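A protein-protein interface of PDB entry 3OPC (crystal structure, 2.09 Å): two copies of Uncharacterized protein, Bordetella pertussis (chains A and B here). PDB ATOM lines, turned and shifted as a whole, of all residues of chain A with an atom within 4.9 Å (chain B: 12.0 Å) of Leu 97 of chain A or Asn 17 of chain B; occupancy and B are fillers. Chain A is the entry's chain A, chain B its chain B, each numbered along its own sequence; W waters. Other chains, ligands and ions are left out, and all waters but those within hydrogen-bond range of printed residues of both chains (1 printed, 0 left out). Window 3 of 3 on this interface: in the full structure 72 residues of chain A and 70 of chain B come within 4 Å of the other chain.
Water W1 bridges the side-chain amide oxygen (OD1) of Asn 100 of chain A and the side-chain amide oxygen (OD1) of Asn 17 of chain B.
Of chain B, only Lys 10 (3.5 Å), Leu 13 (3.7 Å) and Glu 14 (3.3 Å) come within 4 Å of Leu 93 of chain A.
Printed residues of chain B within 4 Å of Trp 94 of chain A: Leu 13 (3.8 Å).
Of chain B, only Asn 17 (3.5 Å) comes within 4 Å of Ala 96 of chain A.
Ala 101 of chain A touches just one residue of chain B: Val 20 (3.7 Å).
Printed residues of chain A within 4 Å of Cys 12 of chain B: Arg 64.
Printed residues of chain A within 4 Å of Leu 13 of chain B: Arg 64, Leu 93, Trp 94 and Leu 97.
Of the printed residues of chain A, Glu 14 of chain B touches Leu 93.
Printed residues of chain A within 4 Å of Glu 16 of chain B: Arg 64 and Leu 97.
Leu 19 of chain B touches none of the printed residues of chain A.
Printed residues of chain A within 4 Å of Val 21 of chain B: Asn 100 (3.97 Å).
Phe 23 of chain B touches none of the printed residues of chain A.
The nearest residue of chain A that does not touch Asn 17 of chain B is Leu 93 of chain A (4.2 Å).
Printed residues of chain B that touch a printed residue of chain A: Leu 9, Lys 10, Cys 12, Leu 13, Glu 14, Glu 16, Asn 17, Val 20, Val 21 and Leu 24.
Printed residues of chain A that touch a printed residue of chain B: Arg 64, Leu 93, Trp 94, Ala 96, Leu 97, Asn 100 and Ala 101.
Hydrophobic or aromatic side chains of chain A that line the printed part of chain B: Leu 93, Trp 94 and Leu 97.
Along chain A the printed residues that touch a printed residue of chain B span positions 64 to 101.
Among the printed residues, 18 pairs touch across the chains.
SG of Cys 12 of chain B sits at hydrogen-bond distance from N of Arg 64 of chain A (3.6 Å).
The guanidinium group of Arg 64 of chain A is in salt-bridge range of the side-chain carboxylate of Glu 16 of chain B, at 2.7 Å.
The backbone NH (N) of Leu 97 of chain A lies close to the side-chain amide nitrogen (ND2) of Asn 17 of chain B.
The side-chain amide nitrogen (ND2) of Asn 17 of chain B lies within hydrogen-bond range of the side-chain amide oxygen (OD1) of Asn 100 of chain A, at 2.8 Å.
Among the printed residues, merely in contact across the chains: Arg 64 of chain A with Leu 9 of chain B (3.8 Å), Arg 64 of chain A with Leu 13 of chain B (3.9 Å), Leu 93 of chain A with Lys 10 of chain B (3.5 Å), Leu 93 of chain A with Leu 13 of chain B (3.7 Å), Leu 93 of chain A with Glu 14 of chain B (3.3 Å), Trp 94 of chain A with Leu 13 of chain B (3.8 Å), Ala 96 of chain A with Asn 17 of chain B (3.5 Å), Leu 97 of chain A with Leu 13 of chain B (3.6 Å), Leu 97 of chain A with Glu 16 of chain B (3.9 Å), Leu 97 of chain A with Val 20 of chain B (3.7 Å), Asn 100 of chain A with Val 20 of chain B (3.5 Å), Asn 100 of chain A with Val 21 of chain B (3.97 Å), Asn 100 of chain A with Leu 24 of chain B (3.998 Å) and Ala 101 of chain A with Val 20 of chain B (3.7 Å).
No position is printed for both chains.
The side-chain amide nitrogen (NE2) of Gln 98 of chain A sits close to the indole nitrogen (NE1) of Trp 94 of chain A (3.2 Å).
The backbone carbonyl oxygen of Ala 96 of chain A lies close to the side-chain amide oxygen of Asn 100 of chain A, at 3.3 Å.
The side-chain amino group (NZ) of Lys 10 of chain B lies within salt-bridge range of the side-chain carboxylate (OE2) of Glu 14 of chain B (2.5 Å).
The side-chain carboxylate of Glu 16 of chain B is in hydrogen-bond range of the side-chain sulfur of Cys 12 of chain B.
The backbone carbonyl oxygen of Val 21 of chain B is in hydrogen-bond range of a ring nitrogen (ND1) of His 25 of chain B (3.4 Å).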
ATOM      1  N   ARG A  64     -25.748 -23.481   3.290  1.00  0.00           N
ATOM      2  CA  ARG A  64     -25.647 -24.808   2.711  1.00  0.00           C
ATOM      3  C   ARG A  64     -26.612 -25.024   1.547  1.00  0.00           C
ATOM      4  O   ARG A  64     -26.202 -25.531   0.505  1.00  0.00           O
ATOM      5  CB  ARG A  64     -25.892 -25.883   3.725  1.00  0.00           C
ATOM      6  CG  ARG A  64     -25.915 -27.269   3.111  1.00  0.00           C
ATOM      7  CD  ARG A  64     -25.309 -28.236   4.104  1.00  0.00           C
ATOM      8  NE  ARG A  64     -25.883 -28.071   5.429  1.00  0.00           N
ATOM      9  CZ  ARG A  64     -26.905 -28.765   5.924  1.00  0.00           C
ATOM     10  NH1 ARG A  64     -27.335 -28.506   7.151  1.00  0.00           N
ATOM     11  NH2 ARG A  64     -27.509 -29.700   5.211  1.00  0.00           N
ATOM     12  N   LEU A  93     -17.952 -35.307   8.309  1.00  0.00           N
ATOM     13  CA  LEU A  93     -18.409 -34.044   8.828  1.00  0.00           C
ATOM     14  C   LEU A  93     -19.932 -33.998   8.761  1.00  0.00           C
ATOM     15  O   LEU A  93     -20.586 -33.663   9.746  1.00  0.00           O
ATOM     16  CB  LEU A  93     -17.730 -32.923   8.034  1.00  0.00           C
ATOM     17  CG  LEU A  93     -17.898 -31.460   8.444  1.00  0.00           C
ATOM     18  CD1 LEU A  93     -17.895 -31.171   9.978  1.00  0.00           C
ATOM     19  CD2 LEU A  93     -16.849 -30.600   7.696  1.00  0.00           C
ATOM     20  N   TRP A  94     -20.494 -34.397   7.620  1.00  0.00           N
ATOM     21  CA  TRP A  94     -21.946 -34.479   7.477  1.00  0.00           C
ATOM     22  C   TRP A  94     -22.565 -35.433   8.470  1.00  0.00           C
ATOM     23  O   TRP A  94     -23.609 -35.138   9.013  1.00  0.00           O
ATOM     24  CB  TRP A  94     -22.325 -34.910   6.054  1.00  0.00           C
ATOM     25  CG  TRP A  94     -23.814 -35.119   5.747  1.00  0.00           C
ATOM     26  CD1 TRP A  94     -24.341 -36.118   4.991  1.00  0.00           C
ATOM     27  CD2 TRP A  94     -24.915 -34.287   6.135  1.00  0.00           C
ATOM     28  NE1 TRP A  94     -25.708 -35.988   4.902  1.00  0.00           N
ATOM     29  CE2 TRP A  94     -26.091 -34.879   5.611  1.00  0.00           C
ATOM     30  CE3 TRP A  94     -25.028 -33.095   6.883  1.00  0.00           C
ATOM     31  CZ2 TRP A  94     -27.351 -34.324   5.790  1.00  0.00           C
ATOM     32  CZ3 TRP A  94     -26.278 -32.560   7.088  1.00  0.00           C
ATOM     33  CH2 TRP A  94     -27.439 -33.169   6.523  1.00  0.00           C
ATOM     34  N   GLN A  95     -21.919 -36.574   8.696  1.00  0.00           N
ATOM     35  CA  GLN A  95     -22.411 -37.549   9.650  1.00  0.00           C
ATOM     36  C   GLN A  95     -22.374 -37.033  11.081  1.00  0.00           C
ATOM     37  O   GLN A  95     -23.316 -37.280  11.831  1.00  0.00           O
ATOM     38  CB  GLN A  95     -21.642 -38.868   9.539  1.00  0.00           C
ATOM     39  CG  GLN A  95     -21.891 -39.559   8.166  1.00  0.00           C
ATOM     40  CD  GLN A  95     -23.377 -39.800   7.927  1.00  0.00           C
ATOM     41  OE1 GLN A  95     -24.106 -40.121   8.870  1.00  0.00           O
ATOM     42  NE2 GLN A  95     -23.843 -39.609   6.683  1.00  0.00           N
ATOM     43  N   ALA A  96     -21.328 -36.300  11.441  1.00  0.00           N
ATOM     44  CA  ALA A  96     -21.224 -35.715  12.784  1.00  0.00           C
ATOM     45  C   ALA A  96     -22.259 -34.603  12.982  1.00  0.00           C
ATOM     46  O   ALA A  96     -22.924 -34.538  14.010  1.00  0.00           O
ATOM     47  CB  ALA A  96     -19.802 -35.186  13.056  1.00  0.00           C
ATOM     48  N   LEU A  97     -22.409 -33.722  12.004  1.00  0.00           N
ATOM     49  CA  LEU A  97     -23.472 -32.721  12.090  1.00  0.00           C
ATOM     50  C   LEU A  97     -24.862 -33.367  12.311  1.00  0.00           C
ATOM     51  O   LEU A  97     -25.635 -32.943  13.188  1.00  0.00           O
ATOM     52  CB  LEU A  97     -23.466 -31.862  10.843  1.00  0.00           C
ATOM     53  CG  LEU A  97     -24.581 -30.833  10.735  1.00  0.00           C
ATOM     54  CD1 LEU A  97     -24.580 -29.956  11.976  1.00  0.00           C
ATOM     55  CD2 LEU A  97     -24.451 -30.012   9.432  1.00  0.00           C
ATOM     56  N   GLN A  98     -25.173 -34.381  11.514  1.00  0.00           N
ATOM     57  CA  GLN A  98     -26.447 -35.070  11.650  1.00  0.00           C
ATOM     58  C   GLN A  98     -26.598 -35.665  13.051  1.00  0.00           C
ATOM     59  O   GLN A  98     -27.658 -35.521  13.670  1.00  0.00           O
ATOM     60  CB  GLN A  98     -26.615 -36.193  10.615  1.00  0.00           C
ATOM     61  CG  GLN A  98     -26.986 -35.684   9.242  1.00  0.00           C
ATOM     62  CD  GLN A  98     -27.148 -36.826   8.259  1.00  0.00           C
ATOM     63  OE1 GLN A  98     -28.275 -37.237   7.955  1.00  0.00           O
ATOM     64  NE2 GLN A  98     -26.022 -37.367   7.778  1.00  0.00           N
ATOM     65  N   ALA A  99     -25.555 -36.311  13.535  1.00  0.00           N
ATOM     66  CA  ALA A  99     -25.638 -36.989  14.809  1.00  0.00           C
ATOM     67  C   ALA A  99     -25.779 -35.945  15.940  1.00  0.00           C
ATOM     68  O   ALA A  99     -26.588 -36.099  16.864  1.00  0.00           O
ATOM     69  CB  ALA A  99     -24.424 -37.897  15.027  1.00  0.00           C
ATOM     70  N   ASN A 100     -24.987 -34.891  15.862  1.00  0.00           N
ATOM     71  CA  ASN A 100     -25.045 -33.808  16.854  1.00  0.00           C
ATOM     72  C   ASN A 100     -26.409 -33.086  16.846  1.00  0.00           C
ATOM     73  O   ASN A 100     -26.941 -32.743  17.898  1.00  0.00           O
ATOM     74  CB  ASN A 100     -23.906 -32.797  16.635  1.00  0.00           C
ATOM     75  CG  ASN A 100     -22.541 -33.335  17.087  1.00  0.00           C
ATOM     76  OD1 ASN A 100     -21.487 -33.011  16.503  1.00  0.00           O
ATOM     77  ND2 ASN A 100     -22.559 -34.132  18.146  1.00  0.00           N
ATOM     78  N   ALA A 101     -26.971 -32.876  15.665  1.00  0.00           N
ATOM     79  CA  ALA A 101     -28.278 -32.259  15.549  1.00  0.00           C
ATOM     80  C   ALA A 101     -29.337 -33.169  16.176  1.00  0.00           C
ATOM     81  O   ALA A 101     -30.238 -32.676  16.829  1.00  0.00           O
ATOM     82  CB  ALA A 101     -28.624 -31.958  14.077  1.00  0.00           C
ATOM     83  N   ALA A 102     -29.237 -34.479  15.988  1.00  0.00           N
ATOM     84  CA  ALA A 102     -30.288 -35.360  16.522  1.00  0.00           C
ATOM     85  C   ALA A 102     -30.230 -35.331  18.046  1.00  0.00           C
ATOM     86  O   ALA A 102     -31.263 -35.222  18.695  1.00  0.00           O
ATOM     87  CB  ALA A 102     -30.160 -36.788  15.968  1.00  0.00           C
ATOM     88  N   ALA B   8     -16.279 -25.049  -0.181  1.00  0.00           N
ATOM     89  CA  ALA B   8     -17.260 -24.165   0.408  1.00  0.00           C
ATOM     90  C   ALA B   8     -18.188 -24.988   1.302  1.00  0.00           C
ATOM     91  O   ALA B   8     -18.607 -24.536   2.366  1.00  0.00           O
ATOM     92  CB  ALA B   8     -18.047 -23.437  -0.656  1.00  0.00           C
ATOM     93  N   LEU B   9     -18.494 -26.201   0.870  1.00  0.00           N
ATOM     94  CA  LEU B   9     -19.439 -27.022   1.612  1.00  0.00           C
ATOM     95  C   LEU B   9     -18.800 -27.512   2.908  1.00  0.00           C
ATOM     96  O   LEU B   9     -19.421 -27.454   3.942  1.00  0.00           O
ATOM     97  CB  LEU B   9     -19.958 -28.165   0.771  1.00  0.00           C
ATOM     98  CG  LEU B   9     -21.032 -29.008   1.454  1.00  0.00           C
ATOM     99  CD1 LEU B   9     -22.270 -28.205   1.872  1.00  0.00           C
ATOM    100  CD2 LEU B   9     -21.435 -30.129   0.514  1.00  0.00           C
ATOM    101  N   LYS B  10     -17.533 -27.923   2.849  1.00  0.00           N
ATOM    102  CA  LYS B  10     -16.813 -28.325   4.051  1.00  0.00           C
ATOM    103  C   LYS B  10     -16.860 -27.202   5.082  1.00  0.00           C
ATOM    104  O   LYS B  10     -17.170 -27.410   6.221  1.00  0.00           O
ATOM    105  CB  LYS B  10     -15.352 -28.676   3.704  1.00  0.00           C
ATOM    106  CG  LYS B  10     -14.433 -29.028   4.910  1.00  0.00           C
ATOM    107  CD  LYS B  10     -13.014 -29.370   4.401  1.00  0.00           C
ATOM    108  CE  LYS B  10     -12.071 -29.795   5.534  1.00  0.00           C
ATOM    109  NZ  LYS B  10     -11.620 -28.623   6.354  1.00  0.00           N
ATOM    110  N   SER B  11     -16.540 -26.003   4.639  1.00  0.00           N
ATOM    111  CA  SER B  11     -16.513 -24.835   5.492  1.00  0.00           C
ATOM    112  C   SER B  11     -17.855 -24.616   6.181  1.00  0.00           C
ATOM    113  O   SER B  11     -17.912 -24.349   7.370  1.00  0.00           O
ATOM    114  CB  SER B  11     -16.141 -23.612   4.652  1.00  0.00           C
ATOM    115  OG  SER B  11     -16.311 -22.428   5.409  1.00  0.00           O
ATOM    116  N   CYS B  12     -18.927 -24.734   5.409  1.00  0.00           N
ATOM    117  CA  CYS B  12     -20.251 -24.527   5.920  1.00  0.00           C
ATOM    118  C   CYS B  12     -20.577 -25.622   6.930  1.00  0.00           C
ATOM    119  O   CYS B  12     -20.995 -25.329   8.036  1.00  0.00           O
ATOM    120  CB  CYS B  12     -21.263 -24.532   4.791  1.00  0.00           C
ATOM    121  SG  CYS B  12     -22.943 -24.217   5.413  1.00  0.00           S
ATOM    122  N   LEU B  13     -20.338 -26.872   6.561  1.00  0.00           N
ATOM    123  CA  LEU B  13     -20.628 -27.978   7.468  1.00  0.00           C
ATOM    124  C   LEU B  13     -19.785 -27.876   8.770  1.00  0.00           C
ATOM    125  O   LEU B  13     -20.288 -28.205   9.835  1.00  0.00           O
ATOM    126  CB  LEU B  13     -20.391 -29.317   6.786  1.00  0.00           C
ATOM    127  CG  LEU B  13     -21.349 -29.839   5.705  1.00  0.00           C
ATOM    128  CD1 LEU B  13     -20.790 -31.108   5.029  1.00  0.00           C
ATOM    129  CD2 LEU B  13     -22.711 -30.139   6.248  1.00  0.00           C
ATOM    130  N   GLU B  14     -18.524 -27.424   8.698  1.00  0.00           N
ATOM    131  CA  GLU B  14     -17.719 -27.235   9.931  1.00  0.00           C
ATOM    132  C   GLU B  14     -18.326 -26.200  10.854  1.00  0.00           C
ATOM    133  O   GLU B  14     -18.451 -26.439  12.077  1.00  0.00           O
ATOM    134  CB  GLU B  14     -16.278 -26.811   9.625  1.00  0.00           C
ATOM    135  CG  GLU B  14     -15.481 -27.902   9.074  1.00  0.00           C
ATOM    136  CD  GLU B  14     -14.167 -27.468   8.457  1.00  0.00           C
ATOM    137  OE1 GLU B  14     -13.905 -26.251   8.279  1.00  0.00           O
ATOM    138  OE2 GLU B  14     -13.392 -28.372   8.138  1.00  0.00           O
ATOM    139  N   ARG B  15     -18.694 -25.052  10.284  1.00  0.00           N
ATOM    140  CA  ARG B  15     -19.275 -23.999  11.092  1.00  0.00           C
ATOM    141  C   ARG B  15     -20.613 -24.430  11.650  1.00  0.00           C
ATOM    142  O   ARG B  15     -20.913 -24.088  12.786  1.00  0.00           O
ATOM    143  CB  ARG B  15     -19.409 -22.686  10.333  1.00  0.00           C
ATOM    144  CG  ARG B  15     -18.072 -22.071  10.066  1.00  0.00           C
ATOM    145  CD  ARG B  15     -18.159 -20.740   9.332  1.00  0.00           C
ATOM    146  NE  ARG B  15     -18.111 -20.943   7.892  1.00  0.00           N
ATOM    147  CZ  ARG B  15     -19.109 -20.711   7.038  1.00  0.00           C
ATOM    148  NH1 ARG B  15     -18.937 -20.932   5.728  1.00  0.00           N
ATOM    149  NH2 ARG B  15     -20.271 -20.242   7.472  1.00  0.00           N
ATOM    150  N   GLU B  16     -21.408 -25.191  10.889  1.00  0.00           N
ATOM    151  CA  GLU B  16     -22.704 -25.645  11.406  1.00  0.00           C
ATOM    152  C   GLU B  16     -22.509 -26.550  12.575  1.00  0.00           C
ATOM    153  O   GLU B  16     -23.167 -26.381  13.616  1.00  0.00           O
ATOM    154  CB  GLU B  16     -23.548 -26.382  10.361  1.00  0.00           C
ATOM    155  CG  GLU B  16     -24.303 -25.480   9.472  1.00  0.00           C
ATOM    156  CD  GLU B  16     -25.020 -26.218   8.344  1.00  0.00           C
ATOM    157  OE1 GLU B  16     -24.361 -26.569   7.339  1.00  0.00           O
ATOM    158  OE2 GLU B  16     -26.235 -26.426   8.464  1.00  0.00           O
ATOM    159  N   ASN B  17     -21.600 -27.504  12.413  1.00  0.00           N
ATOM    160  CA  ASN B  17     -21.349 -28.498  13.445  1.00  0.00           C
ATOM    161  C   ASN B  17     -20.771 -27.861  14.705  1.00  0.00           C
ATOM    162  O   ASN B  17     -21.093 -28.307  15.815  1.00  0.00           O
ATOM    163  CB  ASN B  17     -20.425 -29.599  12.924  1.00  0.00           C
ATOM    164  CG  ASN B  17     -20.272 -30.713  13.895  1.00  0.00           C
ATOM    165  OD1 ASN B  17     -19.166 -30.959  14.389  1.00  0.00           O
ATOM    166  ND2 ASN B  17     -21.360 -31.377  14.226  1.00  0.00           N
ATOM    167  N   ALA B  18     -19.943 -26.832  14.547  1.00  0.00           N
ATOM    168  CA  ALA B  18     -19.460 -26.105  15.720  1.00  0.00           C
ATOM    169  C   ALA B  18     -20.597 -25.355  16.440  1.00  0.00           C
ATOM    170  O   ALA B  18     -20.595 -25.286  17.656  1.00  0.00           O
ATOM    171  CB  ALA B  18     -18.322 -25.177  15.394  1.00  0.00           C
ATOM    172  N   LEU B  19     -21.560 -24.812  15.700  1.00  0.00           N
ATOM    173  CA  LEU B  19     -22.709 -24.173  16.307  1.00  0.00           C
ATOM    174  C   LEU B  19     -23.615 -25.197  16.999  1.00  0.00           C
ATOM    175  O   LEU B  19     -24.115 -24.963  18.097  1.00  0.00           O
ATOM    176  CB  LEU B  19     -23.484 -23.368  15.273  1.00  0.00           C
ATOM    177  CG  LEU B  19     -22.757 -22.084  14.810  1.00  0.00           C
ATOM    178  CD1 LEU B  19     -23.656 -21.321  13.855  1.00  0.00           C
ATOM    179  CD2 LEU B  19     -22.402 -21.197  15.997  1.00  0.00           C
ATOM    180  N   VAL B  20     -23.812 -26.345  16.385  1.00  0.00           N
ATOM    181  CA  VAL B  20     -24.632 -27.351  17.036  1.00  0.00           C
ATOM    182  C   VAL B  20     -23.988 -27.759  18.365  1.00  0.00           C
ATOM    183  O   VAL B  20     -24.680 -27.874  19.395  1.00  0.00           O
ATOM    184  CB  VAL B  20     -24.921 -28.555  16.152  1.00  0.00           C
ATOM    185  CG1 VAL B  20     -25.676 -29.638  16.939  1.00  0.00           C
ATOM    186  CG2 VAL B  20     -25.726 -28.115  14.926  1.00  0.00           C
ATOM    187  N   VAL B  21     -22.677 -27.930  18.353  1.00  0.00           N
ATOM    188  CA  VAL B  21     -21.929 -28.237  19.570  1.00  0.00           C
ATOM    189  C   VAL B  21     -22.080 -27.137  20.606  1.00  0.00           C
ATOM    190  O   VAL B  21     -22.279 -27.438  21.778  1.00  0.00           O
ATOM    191  CB  VAL B  21     -20.420 -28.517  19.302  1.00  0.00           C
ATOM    192  CG1 VAL B  21     -19.650 -28.769  20.632  1.00  0.00           C
ATOM    193  CG2 VAL B  21     -20.245 -29.733  18.359  1.00  0.00           C
ATOM    194  N   GLU B  22     -21.996 -25.869  20.208  1.00  0.00           N
ATOM    195  CA  GLU B  22     -22.211 -24.802  21.188  1.00  0.00           C
ATOM    196  C   GLU B  22     -23.639 -24.899  21.699  1.00  0.00           C
ATOM    197  O   GLU B  22     -23.931 -24.633  22.875  1.00  0.00           O
ATOM    198  CB  GLU B  22     -22.011 -23.423  20.571  1.00  0.00           C
ATOM    199  CG  GLU B  22     -20.626 -23.145  20.053  1.00  0.00           C
ATOM    200  CD  GLU B  22     -20.379 -21.632  19.885  1.00  0.00           C
ATOM    201  OE1 GLU B  22     -20.834 -20.857  20.767  1.00  0.00           O
ATOM    202  OE2 GLU B  22     -19.757 -21.230  18.881  1.00  0.00           O
ATOM    203  N   PHE B  23     -24.548 -25.290  20.803  1.00  0.00           N
ATOM    204  CA  PHE B  23     -25.947 -25.438  21.173  1.00  0.00           C
ATOM    205  C   PHE B  23     -26.159 -26.578  22.194  1.00  0.00           C
ATOM    206  O   PHE B  23     -26.996 -26.460  23.102  1.00  0.00           O
ATOM    207  CB  PHE B  23     -26.782 -25.667  19.911  1.00  0.00           C
ATOM    208  CG  PHE B  23     -28.235 -25.524  20.117  1.00  0.00           C
ATOM    209  CD1 PHE B  23     -28.843 -24.287  20.026  1.00  0.00           C
ATOM    210  CD2 PHE B  23     -29.001 -26.606  20.423  1.00  0.00           C
ATOM    211  CE1 PHE B  23     -30.194 -24.123  20.229  1.00  0.00           C
ATOM    212  CE2 PHE B  23     -30.386 -26.460  20.615  1.00  0.00           C
ATOM    213  CZ  PHE B  23     -30.977 -25.209  20.507  1.00  0.00           C
ATOM    214  N   LEU B  24     -25.410 -27.670  22.049  1.00  0.00           N
ATOM    215  CA  LEU B  24     -25.440 -28.742  23.049  1.00  0.00           C
ATOM    216  C   LEU B  24     -24.903 -28.225  24.399  1.00  0.00           C
ATOM    217  O   LEU B  24     -25.466 -28.538  25.442  1.00  0.00           O
ATOM    218  CB  LEU B  24     -24.652 -29.961  22.597  1.00  0.00           C
ATOM    219  CG  LEU B  24     -25.286 -30.745  21.459  1.00  0.00           C
ATOM    220  CD1 LEU B  24     -24.240 -31.638  20.780  1.00  0.00           C
ATOM    221  CD2 LEU B  24     -26.498 -31.550  21.943  1.00  0.00           C
ATOM    222  N   HIS B  25     -23.869 -27.390  24.375  1.00  0.00           N
ATOM    223  CA  HIS B  25     -23.386 -26.805  25.619  1.00  0.00           C
ATOM    224  C   HIS B  25     -24.438 -25.898  26.282  1.00  0.00           C
ATOM    225  O   HIS B  25     -24.622 -25.974  27.487  1.00  0.00           O
ATOM    226  CB  HIS B  25     -22.071 -26.061  25.404  1.00  0.00           C
ATOM    227  CG  HIS B  25     -20.924 -26.962  25.093  1.00  0.00           C
ATOM    228  ND1 HIS B  25     -19.945 -26.633  24.178  1.00  0.00           N
ATOM    229  CD2 HIS B  25     -20.603 -28.192  25.563  1.00  0.00           C
ATOM    230  CE1 HIS B  25     -19.067 -27.619  24.110  1.00  0.00           C
ATOM    231  NE2 HIS B  25     -19.447 -28.579  24.933  1.00  0.00           N
ATOM    232  N   ALA B  26     -25.128 -25.075  25.490  1.00  0.00           N
ATOM    233  CA  ALA B  26     -26.211 -24.225  26.000  1.00  0.00           C
ATOM    234  C   ALA B  26     -27.356 -25.065  26.545  1.00  0.00           C
ATOM    235  O   ALA B  26     -27.975 -24.696  27.564  1.00  0.00           O
ATOM    236  CB  ALA B  26     -26.739 -23.289  24.948  1.00  0.00           C
ATOM    237  N   LEU B  27     -27.644 -26.174  25.881  1.00  0.00           N
ATOM    238  CA  LEU B  27     -28.657 -27.091  26.396  1.00  0.00           C
ATOM    239  C   LEU B  27     -28.254 -27.677  27.755  1.00  0.00           C
ATOM    240  O   LEU B  27     -29.089 -27.782  28.629  1.00  0.00           O
ATOM    241  CB  LEU B  27     -28.964 -28.213  25.424  1.00  0.00           C
ATOM    242  CG  LEU B  27     -29.777 -27.893  24.175  1.00  0.00           C
ATOM    243  CD1 LEU B  27     -29.560 -29.006  23.154  1.00  0.00           C
ATOM    244  CD2 LEU B  27     -31.245 -27.723  24.465  1.00  0.00           C
ATOM    245  N   GLU B  28     -26.989 -28.048  27.925  1.00  0.00           N
ATOM    246  CA  GLU B  28     -26.516 -28.558  29.229  1.00  0.00           C
ATOM    247  C   GLU B  28     -26.687 -27.494  30.313  1.00  0.00           C
ATOM    248  O   GLU B  28     -27.124 -27.810  31.407  1.00  0.00           O
ATOM    249  CB  GLU B  28     -25.045 -29.010  29.177  1.00  0.00           C
ATOM    250  CG  GLU B  28     -24.892 -30.490  28.760  1.00  0.00           C
ATOM    251  CD  GLU B  28     -23.638 -30.782  27.938  1.00  0.00           C
ATOM    252  OE1 GLU B  28     -22.519 -30.390  28.351  1.00  0.00           O
ATOM    253  OE2 GLU B  28     -23.794 -31.408  26.860  1.00  0.00           O
HETATM  254  O   HOH W   1     -18.482 -32.993  16.552  1.00  0.00           O
